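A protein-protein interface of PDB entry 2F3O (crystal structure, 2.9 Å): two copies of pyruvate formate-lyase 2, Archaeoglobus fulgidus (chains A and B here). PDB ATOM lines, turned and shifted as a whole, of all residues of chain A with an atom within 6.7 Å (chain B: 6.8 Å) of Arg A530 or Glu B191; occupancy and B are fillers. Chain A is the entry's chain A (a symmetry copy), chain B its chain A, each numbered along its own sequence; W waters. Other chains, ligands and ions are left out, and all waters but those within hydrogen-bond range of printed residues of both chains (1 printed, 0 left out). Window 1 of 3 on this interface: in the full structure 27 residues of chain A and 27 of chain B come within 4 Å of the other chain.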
ATOM      1  N   GLU A 191     -35.145  20.926  10.211  1.00  0.00           N
ATOM      2  CA  GLU A 191     -35.182  21.839   9.084  1.00  0.00           C
ATOM      3  C   GLU A 191     -36.112  21.349   8.005  1.00  0.00           C
ATOM      4  O   GLU A 191     -36.994  22.080   7.568  1.00  0.00           O
ATOM      5  CB  GLU A 191     -33.790  22.029   8.522  1.00  0.00           C
ATOM      6  CG  GLU A 191     -33.222  23.387   8.810  1.00  0.00           C
ATOM      7  CD  GLU A 191     -31.703  23.364   8.981  1.00  0.00           C
ATOM      8  OE1 GLU A 191     -31.023  24.176   8.273  1.00  0.00           O
ATOM      9  OE2 GLU A 191     -31.207  22.538   9.812  1.00  0.00           O
ATOM     10  N   PHE A 436     -31.407  27.761  -9.665  1.00  0.00           N
ATOM     11  CA  PHE A 436     -31.629  29.022  -9.028  1.00  0.00           C
ATOM     12  C   PHE A 436     -30.366  29.774  -9.344  1.00  0.00           C
ATOM     13  O   PHE A 436     -29.305  29.475  -8.777  1.00  0.00           O
ATOM     14  CB  PHE A 436     -31.753  28.813  -7.538  1.00  0.00           C
ATOM     15  CG  PHE A 436     -32.518  29.898  -6.823  1.00  0.00           C
ATOM     16  CD1 PHE A 436     -33.705  30.393  -7.343  1.00  0.00           C
ATOM     17  CD2 PHE A 436     -32.086  30.372  -5.582  1.00  0.00           C
ATOM     18  CE1 PHE A 436     -34.427  31.351  -6.660  1.00  0.00           C
ATOM     19  CE2 PHE A 436     -32.805  31.329  -4.904  1.00  0.00           C
ATOM     20  CZ  PHE A 436     -33.977  31.818  -5.450  1.00  0.00           C
ATOM     21  N   SER A 502     -26.653  36.204   0.415  1.00  0.00           N
ATOM     22  CA  SER A 502     -27.365  34.967   0.079  1.00  0.00           C
ATOM     23  C   SER A 502     -27.638  34.143   1.324  1.00  0.00           C
ATOM     24  O   SER A 502     -28.666  33.480   1.454  1.00  0.00           O
ATOM     25  CB  SER A 502     -26.606  34.140  -0.949  1.00  0.00           C
ATOM     26  OG  SER A 502     -27.317  34.139  -2.180  1.00  0.00           O
ATOM     27  N   TYR A 503     -26.694  34.207   2.243  1.00  0.00           N
ATOM     28  CA  TYR A 503     -26.870  33.661   3.555  1.00  0.00           C
ATOM     29  C   TYR A 503     -27.970  34.461   4.270  1.00  0.00           C
ATOM     30  O   TYR A 503     -28.838  33.884   4.936  1.00  0.00           O
ATOM     31  CB  TYR A 503     -25.532  33.748   4.250  1.00  0.00           C
ATOM     32  CG  TYR A 503     -25.501  33.408   5.712  1.00  0.00           C
ATOM     33  CD1 TYR A 503     -26.106  32.254   6.213  1.00  0.00           C
ATOM     34  CD2 TYR A 503     -24.793  34.216   6.595  1.00  0.00           C
ATOM     35  CE1 TYR A 503     -26.037  31.950   7.557  1.00  0.00           C
ATOM     36  CE2 TYR A 503     -24.718  33.921   7.930  1.00  0.00           C
ATOM     37  CZ  TYR A 503     -25.333  32.794   8.418  1.00  0.00           C
ATOM     38  OH  TYR A 503     -25.230  32.531   9.775  1.00  0.00           O
ATOM     39  N   ALA A 506     -31.394  33.448   2.995  1.00  0.00           N
ATOM     40  CA  ALA A 506     -31.702  32.134   3.577  1.00  0.00           C
ATOM     41  C   ALA A 506     -32.174  32.227   5.011  1.00  0.00           C
ATOM     42  O   ALA A 506     -32.980  31.415   5.453  1.00  0.00           O
ATOM     43  CB  ALA A 506     -30.499  31.217   3.494  1.00  0.00           C
ATOM     44  N   GLU A 507     -31.695  33.232   5.725  1.00  0.00           N
ATOM     45  CA  GLU A 507     -32.020  33.346   7.122  1.00  0.00           C
ATOM     46  C   GLU A 507     -33.248  34.163   7.426  1.00  0.00           C
ATOM     47  O   GLU A 507     -33.987  33.808   8.337  1.00  0.00           O
ATOM     48  CB  GLU A 507     -30.842  33.900   7.898  1.00  0.00           C
ATOM     49  CG  GLU A 507     -29.709  32.922   8.021  1.00  0.00           C
ATOM     50  CD  GLU A 507     -30.097  31.685   8.801  1.00  0.00           C
ATOM     51  OE1 GLU A 507     -30.476  31.816   9.986  1.00  0.00           O
ATOM     52  OE2 GLU A 507     -30.000  30.573   8.234  1.00  0.00           O
ATOM     53  N   VAL A 526     -35.568  21.120   1.157  1.00  0.00           N
ATOM     54  CA  VAL A 526     -34.782  22.322   1.478  1.00  0.00           C
ATOM     55  C   VAL A 526     -35.258  23.486   0.644  1.00  0.00           C
ATOM     56  O   VAL A 526     -35.572  23.320  -0.527  1.00  0.00           O
ATOM     57  CB  VAL A 526     -33.221  22.086   1.402  1.00  0.00           C
ATOM     58  CG1 VAL A 526     -32.881  20.832   0.679  1.00  0.00           C
ATOM     59  CG2 VAL A 526     -32.484  23.248   0.813  1.00  0.00           C
ATOM     60  N   ASP A 527     -35.382  24.649   1.272  1.00  0.00           N
ATOM     61  CA  ASP A 527     -35.781  25.868   0.574  1.00  0.00           C
ATOM     62  C   ASP A 527     -34.791  26.279  -0.525  1.00  0.00           C
ATOM     63  O   ASP A 527     -33.595  26.054  -0.405  1.00  0.00           O
ATOM     64  CB  ASP A 527     -35.936  27.021   1.570  1.00  0.00           C
ATOM     65  CG  ASP A 527     -36.623  28.235   0.956  1.00  0.00           C
ATOM     66  OD1 ASP A 527     -37.858  28.182   0.763  1.00  0.00           O
ATOM     67  OD2 ASP A 527     -35.945  29.236   0.643  1.00  0.00           O
ATOM     68  N   VAL A 528     -35.318  26.884  -1.584  1.00  0.00           N
ATOM     69  CA  VAL A 528     -34.544  27.479  -2.659  1.00  0.00           C
ATOM     70  C   VAL A 528     -33.424  28.469  -2.268  1.00  0.00           C
ATOM     71  O   VAL A 528     -32.357  28.480  -2.891  1.00  0.00           O
ATOM     72  CB  VAL A 528     -35.496  28.092  -3.702  1.00  0.00           C
ATOM     73  CG1 VAL A 528     -35.911  29.495  -3.346  1.00  0.00           C
ATOM     74  CG2 VAL A 528     -34.889  27.997  -5.094  1.00  0.00           C
ATOM     75  N   SER A 529     -33.622  29.243  -1.206  1.00  0.00           N
ATOM     76  CA  SER A 529     -32.647  30.224  -0.826  1.00  0.00           C
ATOM     77  C   SER A 529     -31.523  29.585  -0.028  1.00  0.00           C
ATOM     78  O   SER A 529     -30.522  30.226   0.303  1.00  0.00           O
ATOM     79  CB  SER A 529     -33.312  31.299  -0.005  1.00  0.00           C
ATOM     80  OG  SER A 529     -33.727  30.767   1.216  1.00  0.00           O
ATOM     81  N   ARG A 530     -31.694  28.311   0.281  1.00  0.00           N
ATOM     82  CA  ARG A 530     -30.713  27.568   1.045  1.00  0.00           C
ATOM     83  C   ARG A 530     -29.969  26.620   0.075  1.00  0.00           C
ATOM     84  O   ARG A 530     -28.964  26.001   0.420  1.00  0.00           O
ATOM     85  CB  ARG A 530     -31.443  26.838   2.181  1.00  0.00           C
ATOM     86  CG  ARG A 530     -30.612  25.910   3.046  1.00  0.00           C
ATOM     87  CD  ARG A 530     -29.816  26.663   4.085  1.00  0.00           C
ATOM     88  NE  ARG A 530     -30.682  27.296   5.069  1.00  0.00           N
ATOM     89  CZ  ARG A 530     -30.228  28.022   6.083  1.00  0.00           C
ATOM     90  NH1 ARG A 530     -28.912  28.202   6.250  1.00  0.00           N
ATOM     91  NH2 ARG A 530     -31.089  28.562   6.938  1.00  0.00           N
ATOM     92  N   GLY A 531     -30.454  26.529  -1.157  1.00  0.00           N
ATOM     93  CA  GLY A 531     -29.708  25.810  -2.154  1.00  0.00           C
ATOM     94  C   GLY A 531     -30.300  24.527  -2.673  1.00  0.00           C
ATOM     95  O   GLY A 531     -29.610  23.774  -3.329  1.00  0.00           O
ATOM     96  N   GLY A 532     -31.577  24.273  -2.418  1.00  0.00           N
ATOM     97  CA  GLY A 532     -32.219  23.040  -2.871  1.00  0.00           C
ATOM     98  C   GLY A 532     -32.352  22.810  -4.369  1.00  0.00           C
ATOM     99  O   GLY A 532     -32.713  21.711  -4.774  1.00  0.00           O
ATOM    100  N   ALA A 533     -32.072  23.821  -5.202  1.00  0.00           N
ATOM    101  CA  ALA A 533     -32.194  23.670  -6.657  1.00  0.00           C
ATOM    102  C   ALA A 533     -31.081  22.770  -7.166  1.00  0.00           C
ATOM    103  O   ALA A 533     -30.055  22.701  -6.514  1.00  0.00           O
ATOM    104  CB  ALA A 533     -32.111  24.998  -7.312  1.00  0.00           C
ATOM    105  N   ASN A 536     -27.074  25.597  -8.859  1.00  0.00           N
ATOM    106  CA  ASN A 536     -27.117  26.868  -8.114  1.00  0.00           C
ATOM    107  C   ASN A 536     -26.058  27.806  -8.612  1.00  0.00           C
ATOM    108  O   ASN A 536     -24.893  27.459  -8.628  1.00  0.00           O
ATOM    109  CB  ASN A 536     -26.907  26.663  -6.621  1.00  0.00           C
ATOM    110  CG  ASN A 536     -28.124  26.100  -5.939  1.00  0.00           C
ATOM    111  OD1 ASN A 536     -28.911  26.825  -5.322  1.00  0.00           O
ATOM    112  ND2 ASN A 536     -28.301  24.802  -6.059  1.00  0.00           N
ATOM    113  N   PHE A 620     -22.743  30.664  -1.787  1.00  0.00           N
ATOM    114  CA  PHE A 620     -23.257  30.149  -0.543  1.00  0.00           C
ATOM    115  C   PHE A 620     -24.166  28.970  -0.773  1.00  0.00           C
ATOM    116  O   PHE A 620     -24.193  28.036   0.027  1.00  0.00           O
ATOM    117  CB  PHE A 620     -24.036  31.247   0.167  1.00  0.00           C
ATOM    118  CG  PHE A 620     -24.856  30.758   1.326  1.00  0.00           C
ATOM    119  CD1 PHE A 620     -24.249  30.398   2.511  1.00  0.00           C
ATOM    120  CD2 PHE A 620     -26.228  30.660   1.229  1.00  0.00           C
ATOM    121  CE1 PHE A 620     -24.977  29.960   3.569  1.00  0.00           C
ATOM    122  CE2 PHE A 620     -26.961  30.207   2.288  1.00  0.00           C
ATOM    123  CZ  PHE A 620     -26.333  29.861   3.462  1.00  0.00           C
ATOM    124  N   ARG A 621     -24.901  29.007  -1.877  1.00  0.00           N
ATOM    125  CA  ARG A 621     -25.843  27.940  -2.172  1.00  0.00           C
ATOM    126  C   ARG A 621     -25.171  26.729  -2.795  1.00  0.00           C
ATOM    127  O   ARG A 621     -25.850  25.840  -3.283  1.00  0.00           O
ATOM    128  CB  ARG A 621     -27.013  28.421  -3.042  1.00  0.00           C
ATOM    129  CG  ARG A 621     -28.001  29.306  -2.315  1.00  0.00           C
ATOM    130  CD  ARG A 621     -29.066  29.853  -3.249  1.00  0.00           C
ATOM    131  NE  ARG A 621     -28.597  31.040  -3.953  1.00  0.00           N
ATOM    132  CZ  ARG A 621     -28.242  31.068  -5.237  1.00  0.00           C
ATOM    133  NH1 ARG A 621     -28.314  29.973  -5.997  1.00  0.00           N
ATOM    134  NH2 ARG A 621     -27.817  32.209  -5.763  1.00  0.00           N
ATOM    135  N   GLY A 622     -23.850  26.689  -2.810  1.00  0.00           N
ATOM    136  CA  GLY A 622     -23.162  25.444  -3.093  1.00  0.00           C
ATOM    137  C   GLY A 622     -22.852  25.162  -4.537  1.00  0.00           C
ATOM    138  O   GLY A 622     -22.432  24.067  -4.877  1.00  0.00           O
ATOM    139  N   ILE B  40     -26.270  34.426  16.264  1.00  0.00           N
ATOM    140  CA  ILE B  40     -25.086  33.974  17.012  1.00  0.00           C
ATOM    141  C   ILE B  40     -24.203  35.152  17.367  1.00  0.00           C
ATOM    142  O   ILE B  40     -23.568  35.148  18.418  1.00  0.00           O
ATOM    143  CB  ILE B  40     -24.289  32.829  16.277  1.00  0.00           C
ATOM    144  CG1 ILE B  40     -23.248  32.174  17.184  1.00  0.00           C
ATOM    145  CG2 ILE B  40     -23.644  33.322  15.018  1.00  0.00           C
ATOM    146  CD1 ILE B  40     -22.571  30.993  16.564  1.00  0.00           C
ATOM    147  N   LEU B 182     -11.506  33.047   5.430  1.00  0.00           N
ATOM    148  CA  LEU B 182     -12.853  32.813   4.964  1.00  0.00           C
ATOM    149  C   LEU B 182     -13.197  33.880   3.967  1.00  0.00           C
ATOM    150  O   LEU B 182     -13.825  33.610   2.941  1.00  0.00           O
ATOM    151  CB  LEU B 182     -13.833  32.829   6.129  1.00  0.00           C
ATOM    152  CG  LEU B 182     -13.915  31.437   6.740  1.00  0.00           C
ATOM    153  CD1 LEU B 182     -14.808  31.423   7.942  1.00  0.00           C
ATOM    154  CD2 LEU B 182     -14.414  30.478   5.702  1.00  0.00           C
ATOM    155  N   VAL B 187     -16.292  34.106   1.393  1.00  0.00           N
ATOM    156  CA  VAL B 187     -17.324  33.823   2.399  1.00  0.00           C
ATOM    157  C   VAL B 187     -18.509  33.013   1.876  1.00  0.00           C
ATOM    158  O   VAL B 187     -19.647  33.413   2.011  1.00  0.00           O
ATOM    159  CB  VAL B 187     -17.778  35.115   3.132  1.00  0.00           C
ATOM    160  CG1 VAL B 187     -18.623  34.799   4.370  1.00  0.00           C
ATOM    161  CG2 VAL B 187     -16.571  35.899   3.574  1.00  0.00           C
ATOM    162  N   TYR B 188     -18.257  31.872   1.257  1.00  0.00           N
ATOM    163  CA  TYR B 188     -19.382  31.063   0.819  1.00  0.00           C
ATOM    164  C   TYR B 188     -19.895  30.256   2.006  1.00  0.00           C
ATOM    165  O   TYR B 188     -20.997  29.714   1.994  1.00  0.00           O
ATOM    166  CB  TYR B 188     -19.029  30.164  -0.368  1.00  0.00           C
ATOM    167  CG  TYR B 188     -17.930  29.150  -0.135  1.00  0.00           C
ATOM    168  CD1 TYR B 188     -16.599  29.516  -0.242  1.00  0.00           C
ATOM    169  CD2 TYR B 188     -18.228  27.823   0.162  1.00  0.00           C
ATOM    170  CE1 TYR B 188     -15.591  28.626  -0.039  1.00  0.00           C
ATOM    171  CE2 TYR B 188     -17.227  26.900   0.366  1.00  0.00           C
ATOM    172  CZ  TYR B 188     -15.894  27.313   0.260  1.00  0.00           C
ATOM    173  OH  TYR B 188     -14.854  26.424   0.461  1.00  0.00           O
ATOM    174  N   GLU B 189     -19.064  30.204   3.041  1.00  0.00           N
ATOM    175  CA  GLU B 189     -19.344  29.479   4.249  1.00  0.00           C
ATOM    176  C   GLU B 189     -19.839  30.451   5.282  1.00  0.00           C
ATOM    177  O   GLU B 189     -19.196  30.627   6.316  1.00  0.00           O
ATOM    178  CB  GLU B 189     -18.065  28.815   4.748  1.00  0.00           C
ATOM    179  CG  GLU B 189     -17.642  27.640   3.927  1.00  0.00           C
ATOM    180  CD  GLU B 189     -16.203  27.239   4.182  1.00  0.00           C
ATOM    181  OE1 GLU B 189     -15.966  26.304   4.978  1.00  0.00           O
ATOM    182  OE2 GLU B 189     -15.300  27.871   3.577  1.00  0.00           O
ATOM    183  N   GLY B 190     -20.969  31.084   5.003  1.00  0.00           N
ATOM    184  CA  GLY B 190     -21.518  32.092   5.892  1.00  0.00           C
ATOM    185  C   GLY B 190     -21.671  31.699   7.355  1.00  0.00           C
ATOM    186  O   GLY B 190     -21.350  32.499   8.245  1.00  0.00           O
ATOM    187  N   GLU B 191     -22.142  30.468   7.604  1.00  0.00           N
ATOM    188  CA  GLU B 191     -22.377  29.987   8.952  1.00  0.00           C
ATOM    189  C   GLU B 191     -21.101  29.929   9.751  1.00  0.00           C
ATOM    190  O   GLU B 191     -21.028  30.480  10.844  1.00  0.00           O
ATOM    191  CB  GLU B 191     -23.027  28.622   8.912  1.00  0.00           C
ATOM    192  CG  GLU B 191     -24.468  28.645   9.332  1.00  0.00           C
ATOM    193  CD  GLU B 191     -25.307  27.592   8.608  1.00  0.00           C
ATOM    194  OE1 GLU B 191     -26.002  26.804   9.330  1.00  0.00           O
ATOM    195  OE2 GLU B 191     -25.260  27.558   7.338  1.00  0.00           O
ATOM    196  N   LYS B 192     -20.093  29.285   9.173  1.00  0.00           N
ATOM    197  CA  LYS B 192     -18.748  29.238   9.732  1.00  0.00           C
ATOM    198  C   LYS B 192     -18.207  30.644  10.009  1.00  0.00           C
ATOM    199  O   LYS B 192     -17.539  30.874  11.018  1.00  0.00           O
ATOM    200  CB  LYS B 192     -17.810  28.548   8.749  1.00  0.00           C
ATOM    201  CG  LYS B 192     -17.447  27.101   9.021  1.00  0.00           C
ATOM    202  CD  LYS B 192     -16.097  26.822   8.373  1.00  0.00           C
ATOM    203  CE  LYS B 192     -15.532  25.452   8.675  1.00  0.00           C
ATOM    204  NZ  LYS B 192     -16.126  24.423   7.791  1.00  0.00           N
ATOM    205  N   TYR B 193     -18.508  31.579   9.110  1.00  0.00           N
ATOM    206  CA  TYR B 193     -18.099  32.965   9.267  1.00  0.00           C
ATOM    207  C   TYR B 193     -18.756  33.674  10.471  1.00  0.00           C
ATOM    208  O   TYR B 193     -18.074  34.263  11.296  1.00  0.00           O
ATOM    209  CB  TYR B 193     -18.395  33.693   7.972  1.00  0.00           C
ATOM    210  CG  TYR B 193     -17.778  35.063   7.829  1.00  0.00           C
ATOM    211  CD1 TYR B 193     -16.398  35.233   7.783  1.00  0.00           C
ATOM    212  CD2 TYR B 193     -18.583  36.185   7.672  1.00  0.00           C
ATOM    213  CE1 TYR B 193     -15.846  36.496   7.616  1.00  0.00           C
ATOM    214  CE2 TYR B 193     -18.040  37.434   7.496  1.00  0.00           C
ATOM    215  CZ  TYR B 193     -16.680  37.586   7.474  1.00  0.00           C
ATOM    216  OH  TYR B 193     -16.173  38.841   7.313  1.00  0.00           O
ATOM    217  N   SER B 194     -20.074  33.575  10.578  1.00  0.00           N
ATOM    218  CA  SER B 194     -20.818  34.028  11.749  1.00  0.00           C
ATOM    219  C   SER B 194     -20.260  33.466  13.041  1.00  0.00           C
ATOM    220  O   SER B 194     -20.209  34.166  14.058  1.00  0.00           O
ATOM    221  CB  SER B 194     -22.272  33.575  11.638  1.00  0.00           C
ATOM    222  OG  SER B 194     -22.903  34.126  10.500  1.00  0.00           O
ATOM    223  N   PHE B 195     -19.856  32.195  12.994  1.00  0.00           N
ATOM    224  CA  PHE B 195     -19.310  31.521  14.167  1.00  0.00           C
ATOM    225  C   PHE B 195     -18.028  32.178  14.640  1.00  0.00           C
ATOM    226  O   PHE B 195     -17.923  32.581  15.787  1.00  0.00           O
ATOM    227  CB  PHE B 195     -19.037  30.055  13.892  1.00  0.00           C
ATOM    228  CG  PHE B 195     -18.438  29.330  15.054  1.00  0.00           C
ATOM    229  CD1 PHE B 195     -19.247  28.754  16.007  1.00  0.00           C
ATOM    230  CD2 PHE B 195     -17.064  29.221  15.199  1.00  0.00           C
ATOM    231  CE1 PHE B 195     -18.695  28.077  17.081  1.00  0.00           C
ATOM    232  CE2 PHE B 195     -16.509  28.553  16.273  1.00  0.00           C
ATOM    233  CZ  PHE B 195     -17.319  27.982  17.207  1.00  0.00           C
ATOM    234  N   TYR B 196     -17.051  32.277  13.751  1.00  0.00           N
ATOM    235  CA  TYR B 196     -15.789  32.899  14.109  1.00  0.00           C
ATOM    236  C   TYR B 196     -15.920  34.388  14.488  1.00  0.00           C
ATOM    237  O   TYR B 196     -15.199  34.888  15.378  1.00  0.00           O
ATOM    238  CB  TYR B 196     -14.763  32.650  13.015  1.00  0.00           C
ATOM    239  CG  TYR B 196     -14.310  31.202  13.004  1.00  0.00           C
ATOM    240  CD1 TYR B 196     -14.290  30.454  11.826  1.00  0.00           C
ATOM    241  CD2 TYR B 196     -13.935  30.577  14.181  1.00  0.00           C
ATOM    242  CE1 TYR B 196     -13.897  29.133  11.820  1.00  0.00           C
ATOM    243  CE2 TYR B 196     -13.542  29.244  14.191  1.00  0.00           C
ATOM    244  CZ  TYR B 196     -13.524  28.528  13.008  1.00  0.00           C
ATOM    245  OH  TYR B 196     -13.098  27.222  13.026  1.00  0.00           O
ATOM    246  N   GLU B 507     -31.545  27.594  16.920  1.00  0.00           N
ATOM    247  CA  GLU B 507     -32.007  28.726  16.160  1.00  0.00           C
ATOM    248  C   GLU B 507     -32.107  30.014  16.935  1.00  0.00           C
ATOM    249  O   GLU B 507     -31.807  31.065  16.380  1.00  0.00           O
ATOM    250  CB  GLU B 507     -33.342  28.423  15.512  1.00  0.00           C
ATOM    251  CG  GLU B 507     -33.236  27.437  14.385  1.00  0.00           C
ATOM    252  CD  GLU B 507     -32.398  27.960  13.239  1.00  0.00           C
ATOM    253  OE1 GLU B 507     -32.761  29.006  12.657  1.00  0.00           O
ATOM    254  OE2 GLU B 507     -31.382  27.310  12.904  1.00  0.00           O
ATOM    255  N   GLY B 525     -15.846  25.056  13.498  1.00  0.00           N
ATOM    256  CA  GLY B 525     -16.538  26.305  13.249  1.00  0.00           C
ATOM    257  C   GLY B 525     -18.042  26.183  13.279  1.00  0.00           C
ATOM    258  O   GLY B 525     -18.739  26.901  12.567  1.00  0.00           O
ATOM    259  N   VAL B 526     -18.546  25.246  14.082  1.00  0.00           N
ATOM    260  CA  VAL B 526     -19.992  25.092  14.298  1.00  0.00           C
ATOM    261  C   VAL B 526     -20.305  25.177  15.772  1.00  0.00           C
ATOM    262  O   VAL B 526     -19.560  24.660  16.593  1.00  0.00           O
ATOM    263  CB  VAL B 526     -20.595  23.810  13.597  1.00  0.00           C
ATOM    264  CG1 VAL B 526     -19.538  22.849  13.186  1.00  0.00           C
ATOM    265  CG2 VAL B 526     -21.633  23.124  14.430  1.00  0.00           C
ATOM    266  N   ARG B 530     -25.686  23.230  17.609  1.00  0.00           N
ATOM    267  CA  ARG B 530     -25.928  22.804  16.246  1.00  0.00           C
ATOM    268  C   ARG B 530     -25.217  21.447  16.036  1.00  0.00           C
ATOM    269  O   ARG B 530     -25.404  20.768  15.026  1.00  0.00           O
ATOM    270  CB  ARG B 530     -25.436  23.910  15.303  1.00  0.00           C
ATOM    271  CG  ARG B 530     -25.500  23.622  13.815  1.00  0.00           C
ATOM    272  CD  ARG B 530     -26.891  23.812  13.259  1.00  0.00           C
ATOM    273  NE  ARG B 530     -27.304  25.206  13.313  1.00  0.00           N
ATOM    274  CZ  ARG B 530     -28.487  25.635  12.890  1.00  0.00           C
ATOM    275  NH1 ARG B 530     -29.373  24.774  12.375  1.00  0.00           N
ATOM    276  NH2 ARG B 530     -28.782  26.927  12.974  1.00  0.00           N
HETATM  277  O   HOH W   1     -22.430  27.445   2.573  1.00  0.00           O
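The side-chain carboxylate of Glu B191 is in salt-bridge range of the guanidinium group of Arg A530, at 3.9 Å.
The guanidinium group (NH1) of Arg B530 is in salt-bridge range of the side-chain carboxylate (OE2) of Glu A191 (3.9 Å).
OG of Ser B194 sits at hydrogen-bond distance from OH of Tyr A503 (2.9 Å).
The side-chain hydroxyl (OH) of Tyr B188 lies close to the side-chain carboxylate (OE2) of Glu B189, 3.5 Å away.
The side-chain hydroxyl (OG) of Ser B194 is in hydrogen-bond range of the backbone carbonyl oxygen (O) of Gly B190, at 3.2 Å.
The side-chain carboxylate (OE2) of Glu B507 is in salt-bridge range of the guanidinium group (NH2) of Arg B530 (2.6 Å).
OE2 of Glu A507 lies within salt-bridge range of NH2 of Arg A530.
Among the printed residues, pairs that only touch across the chains: Tyr A503 with Gly B190 (3.7 Å), Tyr A503 with Glu B191 (3.9 Å) and Phe A620 with Tyr B188 (3.4 Å).
Glu B191 touches just these residues of chain A: Tyr A503 (3.9 Å) and Arg A530 (3.9 Å).
Printed residues of chain A within 4 Å of Arg B530: Glu A191 (3.9 Å).
Of the printed residues of chain A, Tyr B188 touches Phe A620.
Printed residues of chain A within 4 Å of Gly B190: Tyr A503.
Ser A502 touches none of the printed residues of chain B.
The nearest residue of chain A that does not touch Glu B191 is Phe A620 (4.5 Å).
The nearest printed residue of chain A that does not touch Tyr B188 is Arg A621 (5.5 Å).
Of the 16 printed residues of chain B, 5 touch a printed residue of chain A.
Glu A191 touches Arg B530, and with the chains exchanged Arg A530 touches Glu B191.
Positions printed for both chains: 191, 507, 526 and 530.
Water W1 bridges O of Tyr B188 and O of Phe A620.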
